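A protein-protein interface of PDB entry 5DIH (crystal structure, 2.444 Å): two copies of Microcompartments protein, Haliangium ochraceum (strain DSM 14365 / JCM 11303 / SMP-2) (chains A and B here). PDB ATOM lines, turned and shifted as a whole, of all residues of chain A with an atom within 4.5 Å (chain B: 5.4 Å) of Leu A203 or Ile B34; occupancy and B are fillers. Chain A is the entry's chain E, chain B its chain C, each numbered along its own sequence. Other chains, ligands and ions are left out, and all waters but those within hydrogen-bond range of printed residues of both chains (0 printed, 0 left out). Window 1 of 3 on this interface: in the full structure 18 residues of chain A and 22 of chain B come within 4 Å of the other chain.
The backbone carbonyl oxygen of Phe A205 is in hydrogen-bond range of the backbone NH of Ser B51 (3.1 Å). OG of Ser B51 is in hydrogen-bond range of O of Leu A203, 3.3 Å away.
O of Ala B31 is in hydrogen-bond range of OG1 of Thr B35, 3.1 Å away. The side-chain hydroxyl of Ser B29 lies close to the backbone NH of Ala B31 (3.5 Å). The side-chain hydroxyl of Ser B51 is in hydrogen-bond range of a ring nitrogen (NE2) of His B59, at 3.3 Å.
CB of Ala B31 touches O of Ile A123, 3.7 Å away. Ile A123 touches Ile B34. Ile B34 touches Ile A192. O of Ile B34 touches CD2 of Leu A199 (3.99 Å). Leu A199 touches Asp B38. Leu A203 touches Ile B34. Phe A204 touches Ile B30 (CE2 to CG2, 3.5 Å). Phe A204 touches Ser B51.
Printed residues of chain B within 4 Å of Ile A123: Ala B31 and Ile B34. Leu A203 touches two residues of chain B. Printed residues of chain B within 4 Å of Phe A204: Ile B30 (3.5 Å) and Ser B51 (3.4 Å). Of the printed residues of chain A, Ile B34 touches Ile A123, Ile A192, Leu A199 and Leu A203. Printed residues of chain A within 4 Å of Asp B38: Leu A199. The nearest printed residue of chain A that does not touch Ile B34 is Phe A204 (4.8 Å).
Of the 12 printed residues of chain B, 5 touch a printed residue of chain A. Of the 10 printed residues of chain A, 6 touch a printed residue of chain B. Hydrophobic or aromatic side chains of chain A that line the printed part of chain B: Ile A123, Ile A192, Leu A199, Leu A203, Phe A204 and Phe A205. Along chain A the printed residues that touch a printed residue of chain B span positions 123 to 205. Among the printed residues, no Asp or Glu carboxylate lies within 4 Å of a Lys or Arg side-chain nitrogen of the other chain.
No position is printed for both chains. Of the 10 pairs that touch across the chains among the printed residues, none has its exchanged pair printed and touching as well.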
ATOM      1  N   TRP A 114     -14.038  26.823  31.878  1.00  0.00           N
ATOM      2  CA  TRP A 114     -14.151  27.655  33.070  1.00  0.00           C
ATOM      3  C   TRP A 114     -15.376  28.562  33.000  1.00  0.00           C
ATOM      4  O   TRP A 114     -16.422  28.254  33.573  1.00  0.00           O
ATOM      5  CB  TRP A 114     -12.885  28.496  33.254  1.00  0.00           C
ATOM      6  CG  TRP A 114     -11.637  27.676  33.398  1.00  0.00           C
ATOM      7  CD1 TRP A 114     -11.555  26.366  33.771  1.00  0.00           C
ATOM      8  CD2 TRP A 114     -10.292  28.109  33.158  1.00  0.00           C
ATOM      9  NE1 TRP A 114     -10.244  25.958  33.786  1.00  0.00           N
ATOM     10  CE2 TRP A 114      -9.448  27.009  33.412  1.00  0.00           C
ATOM     11  CE3 TRP A 114      -9.719  29.321  32.756  1.00  0.00           C
ATOM     12  CZ2 TRP A 114      -8.063  27.083  33.277  1.00  0.00           C
ATOM     13  CZ3 TRP A 114      -8.342  29.392  32.623  1.00  0.00           C
ATOM     14  CH2 TRP A 114      -7.531  28.280  32.884  1.00  0.00           C
ATOM     15  N   ILE A 123      -0.766  30.624  37.546  1.00  0.00           N
ATOM     16  CA  ILE A 123      -0.087  29.413  37.113  1.00  0.00           C
ATOM     17  C   ILE A 123       1.201  29.238  37.907  1.00  0.00           C
ATOM     18  O   ILE A 123       2.183  29.948  37.686  1.00  0.00           O
ATOM     19  CB  ILE A 123       0.232  29.435  35.602  1.00  0.00           C
ATOM     20  CG1 ILE A 123      -1.055  29.510  34.773  1.00  0.00           C
ATOM     21  CG2 ILE A 123       1.030  28.200  35.210  1.00  0.00           C
ATOM     22  CD1 ILE A 123      -1.566  30.921  34.521  1.00  0.00           C
ATOM     23  N   THR A 163      -3.115  25.253  38.369  1.00  0.00           N
ATOM     24  CA  THR A 163      -3.801  26.513  38.110  1.00  0.00           C
ATOM     25  C   THR A 163      -4.916  26.753  39.120  1.00  0.00           C
ATOM     26  O   THR A 163      -5.603  25.820  39.532  1.00  0.00           O
ATOM     27  CB  THR A 163      -4.394  26.557  36.686  1.00  0.00           C
ATOM     28  OG1 THR A 163      -5.361  25.512  36.534  1.00  0.00           O
ATOM     29  CG2 THR A 163      -3.301  26.385  35.642  1.00  0.00           C
ATOM     30  N   ILE A 192      -2.532  36.071  35.594  1.00  0.00           N
ATOM     31  CA  ILE A 192      -3.264  36.729  34.517  1.00  0.00           C
ATOM     32  C   ILE A 192      -4.650  37.157  34.989  1.00  0.00           C
ATOM     33  O   ILE A 192      -5.444  36.331  35.438  1.00  0.00           O
ATOM     34  CB  ILE A 192      -3.402  35.816  33.285  1.00  0.00           C
ATOM     35  CG1 ILE A 192      -2.031  35.296  32.851  1.00  0.00           C
ATOM     36  CG2 ILE A 192      -4.082  36.559  32.143  1.00  0.00           C
ATOM     37  CD1 ILE A 192      -2.070  34.434  31.609  1.00  0.00           C
ATOM     38  N   LEU A 199      -7.949  31.084  25.502  1.00  0.00           N
ATOM     39  CA  LEU A 199      -7.224  30.562  26.655  1.00  0.00           C
ATOM     40  C   LEU A 199      -8.178  30.260  27.806  1.00  0.00           C
ATOM     41  O   LEU A 199      -7.915  29.386  28.632  1.00  0.00           O
ATOM     42  CB  LEU A 199      -6.150  31.553  27.110  1.00  0.00           C
ATOM     43  CG  LEU A 199      -4.695  31.141  26.887  1.00  0.00           C
ATOM     44  CD1 LEU A 199      -4.494  30.677  25.462  1.00  0.00           C
ATOM     45  CD2 LEU A 199      -3.756  32.294  27.211  1.00  0.00           C
ATOM     46  N   GLY A 201     -10.824  28.581  29.701  1.00  0.00           N
ATOM     47  CA  GLY A 201     -11.415  27.258  29.642  1.00  0.00           C
ATOM     48  C   GLY A 201     -10.353  26.182  29.533  1.00  0.00           C
ATOM     49  O   GLY A 201     -10.058  25.487  30.504  1.00  0.00           O
ATOM     50  N   ARG A 202      -9.773  26.048  28.344  1.00  0.00           N
ATOM     51  CA  ARG A 202      -8.722  25.065  28.124  1.00  0.00           C
ATOM     52  C   ARG A 202      -7.370  25.755  27.993  1.00  0.00           C
ATOM     53  O   ARG A 202      -7.025  26.280  26.935  1.00  0.00           O
ATOM     54  CB  ARG A 202      -9.016  24.228  26.879  1.00  0.00           C
ATOM     55  CG  ARG A 202      -8.345  22.864  26.880  1.00  0.00           C
ATOM     56  CD  ARG A 202      -8.635  22.120  25.591  1.00  0.00           C
ATOM     57  NE  ARG A 202     -10.064  22.086  25.297  1.00  0.00           N
ATOM     58  CZ  ARG A 202     -10.576  21.716  24.127  1.00  0.00           C
ATOM     59  NH1 ARG A 202     -11.889  21.717  23.946  1.00  0.00           N
ATOM     60  NH2 ARG A 202      -9.774  21.350  23.137  1.00  0.00           N
ATOM     61  N   LEU A 203      -6.611  25.751  29.083  1.00  0.00           N
ATOM     62  CA  LEU A 203      -5.322  26.425  29.129  1.00  0.00           C
ATOM     63  C   LEU A 203      -4.246  25.601  28.430  1.00  0.00           C
ATOM     64  O   LEU A 203      -3.290  26.147  27.879  1.00  0.00           O
ATOM     65  CB  LEU A 203      -4.923  26.695  30.581  1.00  0.00           C
ATOM     66  CG  LEU A 203      -4.209  28.013  30.872  1.00  0.00           C
ATOM     67  CD1 LEU A 203      -5.068  29.192  30.439  1.00  0.00           C
ATOM     68  CD2 LEU A 203      -3.861  28.112  32.349  1.00  0.00           C
ATOM     69  N   PHE A 204      -4.413  24.284  28.452  1.00  0.00           N
ATOM     70  CA  PHE A 204      -3.441  23.377  27.857  1.00  0.00           C
ATOM     71  C   PHE A 204      -4.101  22.466  26.827  1.00  0.00           C
ATOM     72  O   PHE A 204      -5.080  21.784  27.126  1.00  0.00           O
ATOM     73  CB  PHE A 204      -2.755  22.544  28.941  1.00  0.00           C
ATOM     74  CG  PHE A 204      -2.014  23.366  29.956  1.00  0.00           C
ATOM     75  CD1 PHE A 204      -2.666  23.861  31.076  1.00  0.00           C
ATOM     76  CD2 PHE A 204      -0.672  23.653  29.788  1.00  0.00           C
ATOM     77  CE1 PHE A 204      -1.988  24.624  32.009  1.00  0.00           C
ATOM     78  CE2 PHE A 204       0.012  24.412  30.718  1.00  0.00           C
ATOM     79  CZ  PHE A 204      -0.646  24.900  31.829  1.00  0.00           C
ATOM     80  N   PHE A 205      -3.558  22.464  25.614  1.00  0.00           N
ATOM     81  CA  PHE A 205      -4.105  21.658  24.530  1.00  0.00           C
ATOM     82  C   PHE A 205      -3.055  21.401  23.452  1.00  0.00           C
ATOM     83  O   PHE A 205      -1.991  22.021  23.449  1.00  0.00           O
ATOM     84  CB  PHE A 205      -5.336  22.339  23.919  1.00  0.00           C
ATOM     85  CG  PHE A 205      -5.061  23.705  23.347  1.00  0.00           C
ATOM     86  CD1 PHE A 205      -5.102  24.831  24.153  1.00  0.00           C
ATOM     87  CD2 PHE A 205      -4.770  23.861  22.000  1.00  0.00           C
ATOM     88  CE1 PHE A 205      -4.851  26.085  23.629  1.00  0.00           C
ATOM     89  CE2 PHE A 205      -4.519  25.113  21.471  1.00  0.00           C
ATOM     90  CZ  PHE A 205      -4.561  26.225  22.286  1.00  0.00           C
ATOM     91  N   SER B  29       9.922  27.447  30.483  1.00  0.00           N
ATOM     92  CA  SER B  29       9.000  27.538  31.607  1.00  0.00           C
ATOM     93  C   SER B  29       7.549  27.451  31.143  1.00  0.00           C
ATOM     94  O   SER B  29       7.121  28.200  30.263  1.00  0.00           O
ATOM     95  CB  SER B  29       9.227  28.836  32.382  1.00  0.00           C
ATOM     96  OG  SER B  29       8.271  28.983  33.417  1.00  0.00           O
ATOM     97  N   ILE B  30       6.799  26.533  31.743  1.00  0.00           N
ATOM     98  CA  ILE B  30       5.395  26.341  31.401  1.00  0.00           C
ATOM     99  C   ILE B  30       4.552  27.511  31.900  1.00  0.00           C
ATOM    100  O   ILE B  30       3.585  27.916  31.252  1.00  0.00           O
ATOM    101  CB  ILE B  30       4.855  25.025  31.985  1.00  0.00           C
ATOM    102  CG1 ILE B  30       5.734  23.854  31.540  1.00  0.00           C
ATOM    103  CG2 ILE B  30       3.413  24.800  31.561  1.00  0.00           C
ATOM    104  CD1 ILE B  30       5.312  22.523  32.112  1.00  0.00           C
ATOM    105  N   ALA B  31       4.930  28.056  33.052  1.00  0.00           N
ATOM    106  CA  ALA B  31       4.259  29.226  33.601  1.00  0.00           C
ATOM    107  C   ALA B  31       4.495  30.444  32.712  1.00  0.00           C
ATOM    108  O   ALA B  31       3.557  31.166  32.370  1.00  0.00           O
ATOM    109  CB  ALA B  31       4.735  29.497  35.020  1.00  0.00           C
ATOM    110  N   ARG B  32       5.753  30.665  32.342  1.00  0.00           N
ATOM    111  CA  ARG B  32       6.115  31.754  31.441  1.00  0.00           C
ATOM    112  C   ARG B  32       5.476  31.541  30.075  1.00  0.00           C
ATOM    113  O   ARG B  32       5.106  32.498  29.393  1.00  0.00           O
ATOM    114  CB  ARG B  32       7.638  31.859  31.306  1.00  0.00           C
ATOM    115  CG  ARG B  32       8.121  32.973  30.382  1.00  0.00           C
ATOM    116  CD  ARG B  32       8.122  34.327  31.076  1.00  0.00           C
ATOM    117  NE  ARG B  32       9.151  34.413  32.110  1.00  0.00           N
ATOM    118  CZ  ARG B  32      10.380  34.877  31.909  1.00  0.00           C
ATOM    119  NH1 ARG B  32      10.743  35.305  30.707  1.00  0.00           N
ATOM    120  NH2 ARG B  32      11.250  34.916  32.909  1.00  0.00           N
ATOM    121  N   GLY B  33       5.341  30.277  29.688  1.00  0.00           N
ATOM    122  CA  GLY B  33       4.783  29.917  28.397  1.00  0.00           C
ATOM    123  C   GLY B  33       3.352  30.372  28.200  1.00  0.00           C
ATOM    124  O   GLY B  33       2.987  30.865  27.132  1.00  0.00           O
ATOM    125  N   ILE B  34       2.538  30.213  29.235  1.00  0.00           N
ATOM    126  CA  ILE B  34       1.128  30.564  29.155  1.00  0.00           C
ATOM    127  C   ILE B  34       0.937  32.081  29.201  1.00  0.00           C
ATOM    128  O   ILE B  34      -0.123  32.594  28.840  1.00  0.00           O
ATOM    129  CB  ILE B  34       0.325  29.904  30.292  1.00  0.00           C
ATOM    130  CG1 ILE B  34      -1.121  29.661  29.858  1.00  0.00           C
ATOM    131  CG2 ILE B  34       0.402  30.738  31.560  1.00  0.00           C
ATOM    132  CD1 ILE B  34      -1.255  28.645  28.746  1.00  0.00           C
ATOM    133  N   THR B  35       1.969  32.792  29.644  1.00  0.00           N
ATOM    134  CA  THR B  35       1.931  34.249  29.690  1.00  0.00           C
ATOM    135  C   THR B  35       2.295  34.812  28.321  1.00  0.00           C
ATOM    136  O   THR B  35       1.752  35.827  27.884  1.00  0.00           O
ATOM    137  CB  THR B  35       2.892  34.808  30.756  1.00  0.00           C
ATOM    138  OG1 THR B  35       2.661  34.147  32.005  1.00  0.00           O
ATOM    139  CG2 THR B  35       2.683  36.306  30.934  1.00  0.00           C
ATOM    140  N   VAL B  36       3.220  34.136  27.649  1.00  0.00           N
ATOM    141  CA  VAL B  36       3.624  34.505  26.301  1.00  0.00           C
ATOM    142  C   VAL B  36       2.463  34.326  25.325  1.00  0.00           C
ATOM    143  O   VAL B  36       2.245  35.156  24.443  1.00  0.00           O
ATOM    144  CB  VAL B  36       4.833  33.670  25.837  1.00  0.00           C
ATOM    145  CG1 VAL B  36       5.108  33.891  24.359  1.00  0.00           C
ATOM    146  CG2 VAL B  36       6.059  34.011  26.669  1.00  0.00           C
ATOM    147  N   ALA B  37       1.712  33.243  25.502  1.00  0.00           N
ATOM    148  CA  ALA B  37       0.571  32.948  24.642  1.00  0.00           C
ATOM    149  C   ALA B  37      -0.530  33.991  24.795  1.00  0.00           C
ATOM    150  O   ALA B  37      -1.233  34.310  23.838  1.00  0.00           O
ATOM    151  CB  ALA B  37       0.028  31.561  24.944  1.00  0.00           C
ATOM    152  N   ASP B  38      -0.674  34.522  26.005  1.00  0.00           N
ATOM    153  CA  ASP B  38      -1.690  35.534  26.270  1.00  0.00           C
ATOM    154  C   ASP B  38      -1.290  36.885  25.688  1.00  0.00           C
ATOM    155  O   ASP B  38      -2.142  37.669  25.274  1.00  0.00           O
ATOM    156  CB  ASP B  38      -1.942  35.664  27.773  1.00  0.00           C
ATOM    157  CG  ASP B  38      -2.959  36.744  28.099  1.00  0.00           C
ATOM    158  OD1 ASP B  38      -4.168  36.489  27.930  1.00  0.00           O
ATOM    159  OD2 ASP B  38      -2.548  37.846  28.523  1.00  0.00           O
ATOM    160  N   SER B  51      -0.720  24.768  22.931  1.00  0.00           N
ATOM    161  CA  SER B  51      -0.173  25.232  24.200  1.00  0.00           C
ATOM    162  C   SER B  51       0.097  24.012  25.073  1.00  0.00           C
ATOM    163  O   SER B  51      -0.654  23.723  26.005  1.00  0.00           O
ATOM    164  CB  SER B  51      -1.130  26.200  24.895  1.00  0.00           C
ATOM    165  OG  SER B  51      -0.593  26.651  26.126  1.00  0.00           O
ATOM    166  N   HIS B  59       7.971  24.088  27.493  1.00  0.00           N
ATOM    167  CA  HIS B  59       6.649  24.446  26.998  1.00  0.00           C
ATOM    168  C   HIS B  59       6.727  24.789  25.517  1.00  0.00           C
ATOM    169  O   HIS B  59       7.640  25.487  25.079  1.00  0.00           O
ATOM    170  CB  HIS B  59       6.073  25.620  27.789  1.00  0.00           C
ATOM    171  CG  HIS B  59       4.610  25.842  27.562  1.00  0.00           C
ATOM    172  ND1 HIS B  59       3.643  24.996  28.061  1.00  0.00           N
ATOM    173  CD2 HIS B  59       3.949  26.813  26.889  1.00  0.00           C
ATOM    174  CE1 HIS B  59       2.449  25.436  27.706  1.00  0.00           C
ATOM    175  NE2 HIS B  59       2.606  26.538  26.994  1.00  0.00           N
